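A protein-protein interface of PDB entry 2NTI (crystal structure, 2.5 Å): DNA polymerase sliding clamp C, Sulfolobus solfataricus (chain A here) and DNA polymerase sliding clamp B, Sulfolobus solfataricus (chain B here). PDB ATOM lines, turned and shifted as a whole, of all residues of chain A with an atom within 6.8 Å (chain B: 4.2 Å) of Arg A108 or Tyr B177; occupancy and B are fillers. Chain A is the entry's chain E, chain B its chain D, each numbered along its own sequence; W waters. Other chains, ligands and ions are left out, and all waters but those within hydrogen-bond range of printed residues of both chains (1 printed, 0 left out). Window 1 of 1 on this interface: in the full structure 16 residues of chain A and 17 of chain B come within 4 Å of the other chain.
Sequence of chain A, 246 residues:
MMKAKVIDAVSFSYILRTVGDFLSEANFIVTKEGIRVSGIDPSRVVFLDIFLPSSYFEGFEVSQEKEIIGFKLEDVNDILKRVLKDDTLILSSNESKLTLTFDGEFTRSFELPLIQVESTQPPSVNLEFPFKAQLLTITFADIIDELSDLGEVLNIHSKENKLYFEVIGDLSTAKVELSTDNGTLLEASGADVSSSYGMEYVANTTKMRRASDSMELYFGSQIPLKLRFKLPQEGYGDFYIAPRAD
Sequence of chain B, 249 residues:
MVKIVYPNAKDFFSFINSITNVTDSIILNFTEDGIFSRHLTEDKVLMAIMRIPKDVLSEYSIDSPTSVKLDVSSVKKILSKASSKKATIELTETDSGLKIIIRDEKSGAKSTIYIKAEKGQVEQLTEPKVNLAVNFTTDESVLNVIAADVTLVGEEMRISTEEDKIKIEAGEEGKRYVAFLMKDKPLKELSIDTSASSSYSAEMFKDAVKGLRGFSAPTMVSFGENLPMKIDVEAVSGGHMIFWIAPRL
O of Ile B168 is in hydrogen-bond range of N of Ala B179, at 2.9 Å. N of Tyr B177 sits at hydrogen-bond distance from O of Ala B170, 3.0 Å away. O of Arg A82 is in hydrogen-bond range of NH2 of Arg A108, at 2.8 Å. The side-chain carboxylate (OD1) of Asp A87 is in salt-bridge range of the guanidinium group (NH2) of Arg A108 (2.6 Å). The side-chain hydroxyl (OG) of Ser A109 lies within hydrogen-bond range of the side-chain hydroxyl (OG1) of Thr A101. N of Phe A102 is in hydrogen-bond range of O of Arg A108, at 2.8 Å.
Val A83 touches none of the printed residues of chain B. Phe A102 touches none of the printed residues of chain B. Printed residues of chain B within 4 Å of Ser A109: Arg B176 (3.7 Å), Tyr B177 (3.2 Å) and Val B178 (2.7 Å). Of the printed residues of chain B, Glu A111 touches Arg B176 (3.0 Å). Printed residues of chain A within 4 Å of Val B153: Phe A110 (3.7 Å). Of the printed residues of chain A, Arg B176 touches Ser A109 (3.7 Å), Phe A110 (3.3 Å) and Glu A111 (3.0 Å). Tyr B177 touches just these residues of chain A: Arg A108 (3.7 Å), Ser A109 (3.2 Å) and Phe A110 (3.4 Å). The nearest printed residue of chain B that does not touch Arg A108 is Ala B179 (4.2 Å). The nearest residue of chain A that does not touch Tyr B177 is Phe A106 (4.3 Å).
Hydrophobic or aromatic side chains of chain B that line the printed part of chain A: Val B145, Val B153, Tyr B177 and Ala B179. Along chain B the printed residues that touch a printed residue of chain A span positions 145 to 179. Hydrophobic or aromatic side chains of chain A within 4 Å of the printed part of chain B: Leu A84, Phe A106 and Phe A110. Along chain A the printed residues that touch a printed residue of chain B span positions 82 to 111. Among the printed residues, 17 pairs touch across the chains. Among the printed residues, Asp or Glu carboxylates within 4 Å of a Lys or Arg side-chain nitrogen of the other chain: Arg A82 with Asp B149 and Arg A108 with Asp B149.
Water W1 lies within hydrogen-bond range of O of Glu A111 (2.9 Å) and O of Arg B176 (3.3 Å).
The backbone carbonyl oxygen (O) of Val B145 lies within hydrogen-bond range of the guanidinium group (NH1) of Arg A82 (3.3 Å). The side-chain carboxylate (OD1) of Asp B149 lies within salt-bridge range of the guanidinium group (NH1) of Arg A82 (2.7 Å). NH1 of Arg A108 lies within salt-bridge range of OD2 of Asp B149 (3.1 Å). The backbone carbonyl oxygen of Arg B176 is in hydrogen-bond range of the backbone NH of Glu A111 (3.0 Å). The backbone NH (N) of Ser A109 lies within hydrogen-bond range of the backbone carbonyl oxygen (O) of Val B178, 2.7 Å away.
Among the printed residues, merely in contact across the chains: Leu A84 with Val B145 (3.9 Å), Phe A106 with Val B145 (3.8 Å), Thr A107 with Ala B179 (3.1 Å), Arg A108 with Val B145 (3.6 Å), Arg A108 with Tyr B177 (3.7 Å), Arg A108 with Val B178 (3.4 Å), Ser A109 with Arg B176 (3.7 Å), Ser A109 with Tyr B177 (3.2 Å), Phe A110 with Asp B149 (3.3 Å), Phe A110 with Val B153 (3.7 Å), Phe A110 with Arg B176 (3.3 Å) and Phe A110 with Tyr B177 (3.4 Å).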
ATOM      1  N   ILE A  79       8.725 -14.640  23.109  1.00  0.00           N
ATOM      2  CA  ILE A  79       9.732 -15.630  22.768  1.00  0.00           C
ATOM      3  C   ILE A  79      10.895 -15.584  23.756  1.00  0.00           C
ATOM      4  O   ILE A  79      11.376 -16.622  24.210  1.00  0.00           O
ATOM      5  CB  ILE A  79      10.234 -15.450  21.300  1.00  0.00           C
ATOM      6  CG1 ILE A  79       9.050 -15.586  20.324  1.00  0.00           C
ATOM      7  CG2 ILE A  79      11.346 -16.452  20.988  1.00  0.00           C
ATOM      8  CD1 ILE A  79       9.402 -15.366  18.869  1.00  0.00           C
ATOM      9  N   ARG A  82      10.829 -17.303  27.015  1.00  0.00           N
ATOM     10  CA  ARG A  82      10.996 -18.747  26.944  1.00  0.00           C
ATOM     11  C   ARG A  82      12.452 -19.157  27.155  1.00  0.00           C
ATOM     12  O   ARG A  82      12.797 -20.334  27.032  1.00  0.00           O
ATOM     13  CB  ARG A  82      10.504 -19.273  25.588  1.00  0.00           C
ATOM     14  CG  ARG A  82       9.070 -18.852  25.206  1.00  0.00           C
ATOM     15  CD  ARG A  82       8.018 -19.867  25.616  1.00  0.00           C
ATOM     16  NE  ARG A  82       7.974 -20.067  27.060  1.00  0.00           N
ATOM     17  CZ  ARG A  82       8.432 -21.144  27.691  1.00  0.00           C
ATOM     18  NH1 ARG A  82       8.977 -22.145  27.015  1.00  0.00           N
ATOM     19  NH2 ARG A  82       8.341 -21.219  29.011  1.00  0.00           N
ATOM     20  N   VAL A  83      13.292 -18.181  27.481  1.00  0.00           N
ATOM     21  CA  VAL A  83      14.728 -18.383  27.631  1.00  0.00           C
ATOM     22  C   VAL A  83      15.064 -19.231  28.860  1.00  0.00           C
ATOM     23  O   VAL A  83      14.456 -19.083  29.912  1.00  0.00           O
ATOM     24  CB  VAL A  83      15.481 -17.007  27.650  1.00  0.00           C
ATOM     25  CG1 VAL A  83      15.379 -16.317  29.012  1.00  0.00           C
ATOM     26  CG2 VAL A  83      16.914 -17.169  27.229  1.00  0.00           C
ATOM     27  N   LEU A  84      16.028 -20.127  28.708  1.00  0.00           N
ATOM     28  CA  LEU A  84      16.491 -20.951  29.816  1.00  0.00           C
ATOM     29  C   LEU A  84      17.787 -20.414  30.418  1.00  0.00           C
ATOM     30  O   LEU A  84      18.603 -19.802  29.722  1.00  0.00           O
ATOM     31  CB  LEU A  84      16.660 -22.412  29.368  1.00  0.00           C
ATOM     32  CG  LEU A  84      15.347 -23.133  29.007  1.00  0.00           C
ATOM     33  CD1 LEU A  84      15.601 -24.520  28.411  1.00  0.00           C
ATOM     34  CD2 LEU A  84      14.367 -23.213  30.203  1.00  0.00           C
ATOM     35  N   ASP A  87      20.990 -20.749  28.288  1.00  0.00           N
ATOM     36  CA  ASP A  87      20.839 -20.677  26.836  1.00  0.00           C
ATOM     37  C   ASP A  87      21.769 -19.637  26.227  1.00  0.00           C
ATOM     38  O   ASP A  87      21.966 -18.570  26.807  1.00  0.00           O
ATOM     39  CB  ASP A  87      19.400 -20.281  26.465  1.00  0.00           C
ATOM     40  CG  ASP A  87      18.440 -21.470  26.389  1.00  0.00           C
ATOM     41  OD1 ASP A  87      17.218 -21.211  26.322  1.00  0.00           O
ATOM     42  OD2 ASP A  87      18.871 -22.648  26.385  1.00  0.00           O
ATOM     43  N   LEU A 100      14.848 -16.387  16.165  1.00  0.00           N
ATOM     44  CA  LEU A 100      15.502 -16.425  17.465  1.00  0.00           C
ATOM     45  C   LEU A 100      15.733 -17.882  17.834  1.00  0.00           C
ATOM     46  O   LEU A 100      14.777 -18.650  17.967  1.00  0.00           O
ATOM     47  CB  LEU A 100      14.657 -15.709  18.523  1.00  0.00           C
ATOM     48  CG  LEU A 100      14.288 -14.233  18.275  1.00  0.00           C
ATOM     49  CD1 LEU A 100      13.160 -13.757  19.180  1.00  0.00           C
ATOM     50  CD2 LEU A 100      15.481 -13.295  18.423  1.00  0.00           C
ATOM     51  N   THR A 101      17.003 -18.261  17.975  1.00  0.00           N
ATOM     52  CA  THR A 101      17.387 -19.646  18.271  1.00  0.00           C
ATOM     53  C   THR A 101      18.093 -19.759  19.624  1.00  0.00           C
ATOM     54  O   THR A 101      19.168 -19.194  19.832  1.00  0.00           O
ATOM     55  CB  THR A 101      18.299 -20.243  17.163  1.00  0.00           C
ATOM     56  OG1 THR A 101      17.673 -20.115  15.877  1.00  0.00           O
ATOM     57  CG2 THR A 101      18.601 -21.717  17.440  1.00  0.00           C
ATOM     58  N   PHE A 102      17.463 -20.485  20.541  1.00  0.00           N
ATOM     59  CA  PHE A 102      18.042 -20.781  21.842  1.00  0.00           C
ATOM     60  C   PHE A 102      18.820 -22.074  21.769  1.00  0.00           C
ATOM     61  O   PHE A 102      18.371 -23.036  21.154  1.00  0.00           O
ATOM     62  CB  PHE A 102      16.955 -20.905  22.910  1.00  0.00           C
ATOM     63  CG  PHE A 102      16.162 -19.648  23.117  1.00  0.00           C
ATOM     64  CD1 PHE A 102      14.785 -19.642  22.917  1.00  0.00           C
ATOM     65  CD2 PHE A 102      16.790 -18.469  23.525  1.00  0.00           C
ATOM     66  CE1 PHE A 102      14.034 -18.480  23.120  1.00  0.00           C
ATOM     67  CE2 PHE A 102      16.064 -17.304  23.730  1.00  0.00           C
ATOM     68  CZ  PHE A 102      14.677 -17.301  23.517  1.00  0.00           C
ATOM     69  N   ASP A 103      19.986 -22.094  22.409  1.00  0.00           N
ATOM     70  CA  ASP A 103      20.836 -23.276  22.420  1.00  0.00           C
ATOM     71  C   ASP A 103      21.448 -23.508  23.793  1.00  0.00           C
ATOM     72  O   ASP A 103      21.872 -22.564  24.461  1.00  0.00           O
ATOM     73  CB  ASP A 103      21.935 -23.125  21.385  1.00  0.00           C
ATOM     74  CG  ASP A 103      22.523 -24.442  20.968  1.00  0.00           C
ATOM     75  OD1 ASP A 103      23.171 -24.460  19.903  1.00  0.00           O
ATOM     76  OD2 ASP A 103      22.348 -25.462  21.672  1.00  0.00           O
ATOM     77  N   GLY A 104      21.501 -24.774  24.198  1.00  0.00           N
ATOM     78  CA  GLY A 104      22.006 -25.153  25.509  1.00  0.00           C
ATOM     79  C   GLY A 104      21.575 -26.558  25.886  1.00  0.00           C
ATOM     80  O   GLY A 104      22.205 -27.541  25.468  1.00  0.00           O
ATOM     81  N   GLU A 105      20.510 -26.651  26.682  1.00  0.00           N
ATOM     82  CA  GLU A 105      19.908 -27.926  27.026  1.00  0.00           C
ATOM     83  C   GLU A 105      19.616 -28.675  25.742  1.00  0.00           C
ATOM     84  O   GLU A 105      20.133 -29.764  25.519  1.00  0.00           O
ATOM     85  CB  GLU A 105      18.616 -27.704  27.802  1.00  0.00           C
ATOM     86  CG  GLU A 105      18.825 -27.286  29.239  1.00  0.00           C
ATOM     87  CD  GLU A 105      19.250 -28.453  30.095  1.00  0.00           C
ATOM     88  OE1 GLU A 105      20.401 -28.430  30.601  1.00  0.00           O
ATOM     89  OE2 GLU A 105      18.431 -29.401  30.236  1.00  0.00           O
ATOM     90  N   PHE A 106      18.792 -28.069  24.897  1.00  0.00           N
ATOM     91  CA  PHE A 106      18.583 -28.535  23.542  1.00  0.00           C
ATOM     92  C   PHE A 106      18.418 -27.315  22.651  1.00  0.00           C
ATOM     93  O   PHE A 106      18.534 -26.183  23.131  1.00  0.00           O
ATOM     94  CB  PHE A 106      17.381 -29.488  23.457  1.00  0.00           C
ATOM     95  CG  PHE A 106      16.093 -28.935  24.027  1.00  0.00           C
ATOM     96  CD1 PHE A 106      15.913 -28.805  25.401  1.00  0.00           C
ATOM     97  CD2 PHE A 106      15.046 -28.591  23.185  1.00  0.00           C
ATOM     98  CE1 PHE A 106      14.734 -28.315  25.925  1.00  0.00           C
ATOM     99  CE2 PHE A 106      13.848 -28.109  23.698  1.00  0.00           C
ATOM    100  CZ  PHE A 106      13.691 -27.963  25.076  1.00  0.00           C
ATOM    101  N   THR A 107      18.163 -27.533  21.366  1.00  0.00           N
ATOM    102  CA  THR A 107      18.042 -26.439  20.404  1.00  0.00           C
ATOM    103  C   THR A 107      16.586 -26.137  20.059  1.00  0.00           C
ATOM    104  O   THR A 107      15.830 -27.030  19.700  1.00  0.00           O
ATOM    105  CB  THR A 107      18.848 -26.754  19.131  1.00  0.00           C
ATOM    106  OG1 THR A 107      20.156 -27.204  19.516  1.00  0.00           O
ATOM    107  CG2 THR A 107      18.991 -25.513  18.246  1.00  0.00           C
ATOM    108  N   ARG A 108      16.210 -24.866  20.173  1.00  0.00           N
ATOM    109  CA  ARG A 108      14.827 -24.405  19.950  1.00  0.00           C
ATOM    110  C   ARG A 108      14.859 -23.142  19.113  1.00  0.00           C
ATOM    111  O   ARG A 108      15.649 -22.235  19.386  1.00  0.00           O
ATOM    112  CB  ARG A 108      14.133 -24.091  21.280  1.00  0.00           C
ATOM    113  CG  ARG A 108      14.361 -25.124  22.347  1.00  0.00           C
ATOM    114  CD  ARG A 108      13.694 -24.763  23.643  1.00  0.00           C
ATOM    115  NE  ARG A 108      14.472 -23.847  24.471  1.00  0.00           N
ATOM    116  CZ  ARG A 108      13.977 -22.750  25.038  1.00  0.00           C
ATOM    117  NH1 ARG A 108      12.698 -22.426  24.867  1.00  0.00           N
ATOM    118  NH2 ARG A 108      14.758 -21.990  25.796  1.00  0.00           N
ATOM    119  N   SER A 109      13.980 -23.063  18.122  1.00  0.00           N
ATOM    120  CA  SER A 109      14.045 -21.984  17.153  1.00  0.00           C
ATOM    121  C   SER A 109      12.671 -21.399  16.867  1.00  0.00           C
ATOM    122  O   SER A 109      11.742 -22.136  16.546  1.00  0.00           O
ATOM    123  CB  SER A 109      14.655 -22.518  15.866  1.00  0.00           C
ATOM    124  OG  SER A 109      15.538 -21.585  15.311  1.00  0.00           O
ATOM    125  N   PHE A 110      12.547 -20.076  16.984  1.00  0.00           N
ATOM    126  CA  PHE A 110      11.283 -19.387  16.723  1.00  0.00           C
ATOM    127  C   PHE A 110      11.439 -18.448  15.528  1.00  0.00           C
ATOM    128  O   PHE A 110      12.490 -17.844  15.338  1.00  0.00           O
ATOM    129  CB  PHE A 110      10.835 -18.577  17.944  1.00  0.00           C
ATOM    130  CG  PHE A 110      10.592 -19.394  19.193  1.00  0.00           C
ATOM    131  CD1 PHE A 110      11.658 -19.761  20.031  1.00  0.00           C
ATOM    132  CD2 PHE A 110       9.294 -19.761  19.558  1.00  0.00           C
ATOM    133  CE1 PHE A 110      11.438 -20.512  21.210  1.00  0.00           C
ATOM    134  CE2 PHE A 110       9.048 -20.513  20.731  1.00  0.00           C
ATOM    135  CZ  PHE A 110      10.125 -20.882  21.561  1.00  0.00           C
ATOM    136  N   GLU A 111      10.390 -18.322  14.724  1.00  0.00           N
ATOM    137  CA  GLU A 111      10.400 -17.421  13.573  1.00  0.00           C
ATOM    138  C   GLU A 111       9.277 -16.414  13.695  1.00  0.00           C
ATOM    139  O   GLU A 111       8.136 -16.783  13.959  1.00  0.00           O
ATOM    140  CB  GLU A 111      10.227 -18.190  12.258  1.00  0.00           C
ATOM    141  CG  GLU A 111      11.305 -19.216  11.979  1.00  0.00           C
ATOM    142  CD  GLU A 111      11.226 -19.819  10.579  1.00  0.00           C
ATOM    143  OE1 GLU A 111      10.103 -19.984  10.043  1.00  0.00           O
ATOM    144  OE2 GLU A 111      12.303 -20.133  10.016  1.00  0.00           O
ATOM    145  N   VAL B 145       9.011 -27.176  28.824  1.00  0.00           N
ATOM    146  CA  VAL B 145       9.595 -26.127  27.983  1.00  0.00           C
ATOM    147  C   VAL B 145       8.995 -26.224  26.590  1.00  0.00           C
ATOM    148  O   VAL B 145       8.474 -25.240  26.058  1.00  0.00           O
ATOM    149  CB  VAL B 145      11.140 -26.228  27.902  1.00  0.00           C
ATOM    150  CG1 VAL B 145      11.701 -25.285  26.842  1.00  0.00           C
ATOM    151  CG2 VAL B 145      11.754 -25.915  29.253  1.00  0.00           C
ATOM    152  N   ASP B 149       6.528 -23.680  24.551  1.00  0.00           N
ATOM    153  CA  ASP B 149       6.989 -23.184  23.267  1.00  0.00           C
ATOM    154  C   ASP B 149       5.939 -23.384  22.177  1.00  0.00           C
ATOM    155  O   ASP B 149       5.598 -22.439  21.466  1.00  0.00           O
ATOM    156  CB  ASP B 149       8.281 -23.902  22.853  1.00  0.00           C
ATOM    157  CG  ASP B 149       9.483 -23.494  23.683  1.00  0.00           C
ATOM    158  OD1 ASP B 149       9.407 -22.479  24.410  1.00  0.00           O
ATOM    159  OD2 ASP B 149      10.519 -24.185  23.601  1.00  0.00           O
ATOM    160  N   VAL B 150       5.437 -24.618  22.043  1.00  0.00           N
ATOM    161  CA  VAL B 150       4.517 -24.942  20.941  1.00  0.00           C
ATOM    162  C   VAL B 150       3.168 -24.261  21.077  1.00  0.00           C
ATOM    163  O   VAL B 150       2.621 -23.788  20.081  1.00  0.00           O
ATOM    164  CB  VAL B 150       4.368 -26.469  20.616  1.00  0.00           C
ATOM    165  CG1 VAL B 150       5.735 -27.101  20.325  1.00  0.00           C
ATOM    166  CG2 VAL B 150       3.640 -27.233  21.704  1.00  0.00           C
ATOM    167  N   VAL B 153       3.172 -20.765  19.826  1.00  0.00           N
ATOM    168  CA  VAL B 153       3.292 -20.626  18.384  1.00  0.00           C
ATOM    169  C   VAL B 153       2.064 -21.149  17.607  1.00  0.00           C
ATOM    170  O   VAL B 153       1.712 -20.614  16.554  1.00  0.00           O
ATOM    171  CB  VAL B 153       4.606 -21.296  17.903  1.00  0.00           C
ATOM    172  CG1 VAL B 153       4.690 -21.324  16.426  1.00  0.00           C
ATOM    173  CG2 VAL B 153       5.803 -20.556  18.470  1.00  0.00           C
ATOM    174  N   ILE B 168      10.708 -31.495  16.595  1.00  0.00           N
ATOM    175  CA  ILE B 168       9.408 -30.986  16.999  1.00  0.00           C
ATOM    176  C   ILE B 168       9.112 -29.688  16.272  1.00  0.00           C
ATOM    177  O   ILE B 168       9.951 -28.787  16.267  1.00  0.00           O
ATOM    178  CB  ILE B 168       9.344 -30.764  18.519  1.00  0.00           C
ATOM    179  CG1 ILE B 168       9.596 -32.093  19.228  1.00  0.00           C
ATOM    180  CG2 ILE B 168       7.995 -30.174  18.920  1.00  0.00           C
ATOM    181  CD1 ILE B 168       9.651 -31.995  20.697  1.00  0.00           C
ATOM    182  N   GLU B 169       7.933 -29.607  15.650  1.00  0.00           N
ATOM    183  CA  GLU B 169       7.525 -28.429  14.886  1.00  0.00           C
ATOM    184  C   GLU B 169       6.173 -27.916  15.334  1.00  0.00           C
ATOM    185  O   GLU B 169       5.346 -28.689  15.818  1.00  0.00           O
ATOM    186  CB  GLU B 169       7.478 -28.724  13.387  1.00  0.00           C
ATOM    187  CG  GLU B 169       8.836 -28.844  12.740  1.00  0.00           C
ATOM    188  CD  GLU B 169       8.774 -29.406  11.320  1.00  0.00           C
ATOM    189  OE1 GLU B 169       9.067 -28.639  10.372  1.00  0.00           O
ATOM    190  OE2 GLU B 169       8.443 -30.610  11.148  1.00  0.00           O
ATOM    191  N   ALA B 170       5.958 -26.608  15.165  1.00  0.00           N
ATOM    192  CA  ALA B 170       4.673 -25.974  15.447  1.00  0.00           C
ATOM    193  C   ALA B 170       4.490 -24.697  14.629  1.00  0.00           C
ATOM    194  O   ALA B 170       5.451 -24.147  14.099  1.00  0.00           O
ATOM    195  CB  ALA B 170       4.529 -25.686  16.941  1.00  0.00           C
ATOM    196  N   ARG B 176       6.721 -19.815  13.438  1.00  0.00           N
ATOM    197  CA  ARG B 176       7.072 -21.230  13.484  1.00  0.00           C
ATOM    198  C   ARG B 176       7.966 -21.554  14.667  1.00  0.00           C
ATOM    199  O   ARG B 176       8.588 -20.679  15.255  1.00  0.00           O
ATOM    200  CB  ARG B 176       7.766 -21.665  12.189  1.00  0.00           C
ATOM    201  CG  ARG B 176       7.003 -21.379  10.906  1.00  0.00           C
ATOM    202  CD  ARG B 176       5.757 -22.243  10.760  1.00  0.00           C
ATOM    203  NE  ARG B 176       4.923 -21.744   9.656  1.00  0.00           N
ATOM    204  CZ  ARG B 176       3.965 -22.465   9.060  1.00  0.00           C
ATOM    205  NH1 ARG B 176       3.697 -23.747   9.446  1.00  0.00           N
ATOM    206  NH2 ARG B 176       3.276 -21.899   8.062  1.00  0.00           N
ATOM    207  N   TYR B 177       8.016 -22.833  15.001  1.00  0.00           N
ATOM    208  CA  TYR B 177       8.852 -23.329  16.072  1.00  0.00           C
ATOM    209  C   TYR B 177       9.489 -24.634  15.628  1.00  0.00           C
ATOM    210  O   TYR B 177       8.812 -25.497  15.074  1.00  0.00           O
ATOM    211  CB  TYR B 177       8.015 -23.563  17.319  1.00  0.00           C
ATOM    212  CG  TYR B 177       8.759 -24.222  18.448  1.00  0.00           C
ATOM    213  CD1 TYR B 177       9.677 -23.503  19.210  1.00  0.00           C
ATOM    214  CD2 TYR B 177       8.547 -25.563  18.762  1.00  0.00           C
ATOM    215  CE1 TYR B 177      10.361 -24.103  20.249  1.00  0.00           C
ATOM    216  CE2 TYR B 177       9.222 -26.176  19.805  1.00  0.00           C
ATOM    217  CZ  TYR B 177      10.125 -25.439  20.545  1.00  0.00           C
ATOM    218  OH  TYR B 177      10.801 -26.017  21.593  1.00  0.00           O
ATOM    219  N   VAL B 178      10.790 -24.769  15.865  1.00  0.00           N
ATOM    220  CA  VAL B 178      11.488 -26.016  15.602  1.00  0.00           C
ATOM    221  C   VAL B 178      12.397 -26.309  16.771  1.00  0.00           C
ATOM    222  O   VAL B 178      13.147 -25.440  17.195  1.00  0.00           O
ATOM    223  CB  VAL B 178      12.361 -25.956  14.314  1.00  0.00           C
ATOM    224  CG1 VAL B 178      12.846 -27.346  13.936  1.00  0.00           C
ATOM    225  CG2 VAL B 178      11.596 -25.351  13.137  1.00  0.00           C
ATOM    226  N   ALA B 179      12.322 -27.523  17.299  1.00  0.00           N
ATOM    227  CA  ALA B 179      13.256 -27.948  18.328  1.00  0.00           C
ATOM    228  C   ALA B 179      13.844 -29.315  17.995  1.00  0.00           C
ATOM    229  O   ALA B 179      13.196 -30.139  17.350  1.00  0.00           O
ATOM    230  CB  ALA B 179      12.590 -27.956  19.678  1.00  0.00           C
HETATM  231  O   HOH W   1       7.497 -17.818  16.556  1.00  0.00           O
